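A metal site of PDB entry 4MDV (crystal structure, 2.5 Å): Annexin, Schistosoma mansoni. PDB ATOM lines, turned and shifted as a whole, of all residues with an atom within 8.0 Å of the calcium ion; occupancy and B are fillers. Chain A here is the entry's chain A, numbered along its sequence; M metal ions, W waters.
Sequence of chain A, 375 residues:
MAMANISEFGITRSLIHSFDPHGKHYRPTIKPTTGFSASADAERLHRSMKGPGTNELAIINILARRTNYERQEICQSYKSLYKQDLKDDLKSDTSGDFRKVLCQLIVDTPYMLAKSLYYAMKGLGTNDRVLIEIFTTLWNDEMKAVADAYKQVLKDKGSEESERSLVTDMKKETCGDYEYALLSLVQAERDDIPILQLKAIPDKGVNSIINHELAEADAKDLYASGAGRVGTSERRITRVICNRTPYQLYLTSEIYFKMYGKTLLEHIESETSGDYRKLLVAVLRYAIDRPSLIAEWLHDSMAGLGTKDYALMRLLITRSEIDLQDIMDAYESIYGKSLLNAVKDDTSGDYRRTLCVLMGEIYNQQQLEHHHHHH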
ATOM      1  N   HIS A  46     -10.002  27.386  -3.775  1.00  0.00           N
ATOM      2  CA  HIS A  46      -9.920  27.600  -2.326  1.00  0.00           C
ATOM      3  C   HIS A  46     -11.141  28.362  -1.831  1.00  0.00           C
ATOM      4  O   HIS A  46     -11.750  28.003  -0.814  1.00  0.00           O
ATOM      5  CB  HIS A  46      -8.690  28.414  -1.946  1.00  0.00           C
ATOM      6  CG  HIS A  46      -8.861  29.162  -0.661  1.00  0.00           C
ATOM      7  ND1 HIS A  46      -9.333  30.454  -0.608  1.00  0.00           N
ATOM      8  CD2 HIS A  46      -8.665  28.778   0.626  1.00  0.00           C
ATOM      9  CE1 HIS A  46      -9.407  30.847   0.648  1.00  0.00           C
ATOM     10  NE2 HIS A  46      -9.007  29.852   1.420  1.00  0.00           N
ATOM     11  N   ARG A  47     -11.464  29.434  -2.533  1.00  0.00           N
ATOM     12  CA  ARG A  47     -12.635  30.229  -2.252  1.00  0.00           C
ATOM     13  C   ARG A  47     -13.844  29.310  -2.168  1.00  0.00           C
ATOM     14  O   ARG A  47     -14.597  29.346  -1.197  1.00  0.00           O
ATOM     15  CB  ARG A  47     -12.808  31.264  -3.360  1.00  0.00           C
ATOM     16  CG  ARG A  47     -14.170  31.925  -3.451  1.00  0.00           C
ATOM     17  CD  ARG A  47     -14.101  33.232  -4.274  1.00  0.00           C
ATOM     18  NE  ARG A  47     -13.088  33.187  -5.338  1.00  0.00           N
ATOM     19  CZ  ARG A  47     -11.945  33.848  -5.305  1.00  0.00           C
ATOM     20  NH1 ARG A  47     -11.659  34.620  -4.265  1.00  0.00           N
ATOM     21  NH2 ARG A  47     -11.074  33.763  -6.313  1.00  0.00           N
ATOM     22  N   SER A  48     -13.995  28.455  -3.178  1.00  0.00           N
ATOM     23  CA  SER A  48     -15.203  27.651  -3.324  1.00  0.00           C
ATOM     24  C   SER A  48     -15.437  26.639  -2.213  1.00  0.00           C
ATOM     25  O   SER A  48     -16.513  26.028  -2.146  1.00  0.00           O
ATOM     26  CB  SER A  48     -15.288  27.011  -4.705  1.00  0.00           C
ATOM     27  OG  SER A  48     -15.728  27.989  -5.630  1.00  0.00           O
ATOM     28  N   MET A  49     -14.447  26.490  -1.335  1.00  0.00           N
ATOM     29  CA  MET A  49     -14.552  25.597  -0.194  1.00  0.00           C
ATOM     30  C   MET A  49     -14.744  26.355   1.131  1.00  0.00           C
ATOM     31  O   MET A  49     -14.917  25.743   2.192  1.00  0.00           O
ATOM     32  CB  MET A  49     -13.327  24.683  -0.161  1.00  0.00           C
ATOM     33  CG  MET A  49     -13.278  23.754  -1.365  1.00  0.00           C
ATOM     34  SD  MET A  49     -11.910  22.582  -1.313  1.00  0.00           S
ATOM     35  CE  MET A  49     -10.561  23.592  -1.931  1.00  0.00           C
ATOM     36  N   LYS A  50     -14.740  27.679   1.052  1.00  0.00           N
ATOM     37  CA  LYS A  50     -14.999  28.504   2.227  1.00  0.00           C
ATOM     38  C   LYS A  50     -16.427  28.282   2.711  1.00  0.00           C
ATOM     39  O   LYS A  50     -17.272  27.782   1.971  1.00  0.00           O
ATOM     40  N   GLY A  51     -16.683  28.643   3.958  1.00  0.00           N
ATOM     41  CA  GLY A  51     -18.003  28.478   4.536  1.00  0.00           C
ATOM     42  C   GLY A  51     -18.231  27.067   5.020  1.00  0.00           C
ATOM     43  O   GLY A  51     -17.375  26.197   4.843  1.00  0.00           O
ATOM     44  N   PRO A  52     -19.395  26.815   5.638  1.00  0.00           N
ATOM     45  CA  PRO A  52     -19.780  25.510   6.175  1.00  0.00           C
ATOM     46  C   PRO A  52     -20.048  24.506   5.061  1.00  0.00           C
ATOM     47  O   PRO A  52     -19.892  23.293   5.236  1.00  0.00           O
ATOM     48  CB  PRO A  52     -21.105  25.823   6.890  1.00  0.00           C
ATOM     49  CG  PRO A  52     -21.684  26.945   6.090  1.00  0.00           C
ATOM     50  CD  PRO A  52     -20.498  27.790   5.704  1.00  0.00           C
ATOM     51  N   GLY A  53     -20.482  25.037   3.915  1.00  0.00           N
ATOM     52  CA  GLY A  53     -20.815  24.212   2.771  1.00  0.00           C
ATOM     53  C   GLY A  53     -19.798  24.312   1.643  1.00  0.00           C
ATOM     54  O   GLY A  53     -18.621  24.652   1.845  1.00  0.00           O
ATOM     55  N   THR A  54     -20.257  24.001   0.436  1.00  0.00           N
ATOM     56  CA  THR A  54     -19.348  23.955  -0.690  1.00  0.00           C
ATOM     57  C   THR A  54     -20.041  24.329  -1.983  1.00  0.00           C
ATOM     58  O   THR A  54     -21.210  23.996  -2.208  1.00  0.00           O
ATOM     59  CB  THR A  54     -18.717  22.573  -0.868  1.00  0.00           C
ATOM     60  OG1 THR A  54     -17.681  22.405   0.109  1.00  0.00           O
ATOM     61  CG2 THR A  54     -18.139  22.431  -2.269  1.00  0.00           C
ATOM     62  N   ASN A  55     -19.288  25.030  -2.817  1.00  0.00           N
ATOM     63  CA  ASN A  55     -19.712  25.399  -4.154  1.00  0.00           C
ATOM     64  C   ASN A  55     -19.222  24.332  -5.116  1.00  0.00           C
ATOM     65  O   ASN A  55     -18.176  24.485  -5.772  1.00  0.00           O
ATOM     66  CB  ASN A  55     -19.151  26.775  -4.522  1.00  0.00           C
ATOM     67  CG  ASN A  55     -19.835  27.404  -5.730  1.00  0.00           C
ATOM     68  OD1 ASN A  55     -20.206  26.724  -6.700  1.00  0.00           O
ATOM     69  ND2 ASN A  55     -20.005  28.720  -5.674  1.00  0.00           N
ATOM     70  N   ASP A  89      -7.993  19.007   1.052  1.00  0.00           N
ATOM     71  CA  ASP A  89      -9.034  20.012   1.209  1.00  0.00           C
ATOM     72  C   ASP A  89     -10.312  19.664   0.434  1.00  0.00           C
ATOM     73  O   ASP A  89     -11.427  19.991   0.858  1.00  0.00           O
ATOM     74  CB  ASP A  89      -8.531  21.412   0.838  1.00  0.00           C
ATOM     75  CG  ASP A  89      -7.663  22.041   1.940  1.00  0.00           C
ATOM     76  OD1 ASP A  89      -7.945  21.775   3.140  1.00  0.00           O
ATOM     77  OD2 ASP A  89      -6.695  22.780   1.598  1.00  0.00           O
ATOM     78  N   SER A  92     -12.099  16.597   2.292  1.00  0.00           N
ATOM     79  CA  SER A  92     -12.794  16.938   3.524  1.00  0.00           C
ATOM     80  C   SER A  92     -13.997  17.841   3.270  1.00  0.00           C
ATOM     81  O   SER A  92     -14.900  17.959   4.120  1.00  0.00           O
ATOM     82  CB  SER A  92     -11.818  17.557   4.543  1.00  0.00           C
ATOM     83  OG  SER A  92     -11.235  18.752   4.068  1.00  0.00           O
ATOM     84  N   ASP A  93     -14.032  18.444   2.092  1.00  0.00           N
ATOM     85  CA  ASP A  93     -15.180  19.277   1.690  1.00  0.00           C
ATOM     86  C   ASP A  93     -16.269  18.550   0.905  1.00  0.00           C
ATOM     87  O   ASP A  93     -17.353  19.099   0.683  1.00  0.00           O
ATOM     88  CB  ASP A  93     -14.700  20.493   0.895  1.00  0.00           C
ATOM     89  CG  ASP A  93     -14.726  21.760   1.714  1.00  0.00           C
ATOM     90  OD1 ASP A  93     -13.767  21.979   2.505  1.00  0.00           O
ATOM     91  OD2 ASP A  93     -15.703  22.524   1.596  1.00  0.00           O
ATOM     92  N   THR A  94     -16.010  17.314   0.509  1.00  0.00           N
ATOM     93  CA  THR A  94     -16.978  16.579  -0.282  1.00  0.00           C
ATOM     94  C   THR A  94     -17.141  15.140   0.247  1.00  0.00           C
ATOM     95  O   THR A  94     -16.442  14.740   1.186  1.00  0.00           O
ATOM     96  CB  THR A  94     -16.558  16.627  -1.776  1.00  0.00           C
ATOM     97  OG1 THR A  94     -15.461  15.730  -2.022  1.00  0.00           O
ATOM     98  CG2 THR A  94     -16.120  18.054  -2.134  1.00  0.00           C
HETATM   99 CA    CA M   1     -16.529  24.131   3.154  1.00  0.00          CA
HETATM  100  O   HOH W   1     -14.441  24.254   4.796  1.00  0.00           O
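The backbone carbonyl oxygen of Asp 93 lies within hydrogen-bond range of the side-chain hydroxyl of Thr 54.
Merely in contact with the calcium ion: Thr 54 (3.7 Å) and Lys 50 (3.9 Å).
Within 4 Å of the calcium ion: Met 49, Lys 50, Gly 51, Gly 53, Thr 54 and Asp 93.
The nearest printed residue that does not touch the calcium ion is Pro 52 (4.02 Å).
The calcium ion is bound by OD2 of Asp 93 (2.4 Å), O of Met 49 (2.5 Å), O of Gly 53 (2.5 Å), water W1 (2.7 Å) and O of Gly 51 (2.8 Å).
The calcium ion has five donor atoms within binding distance.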
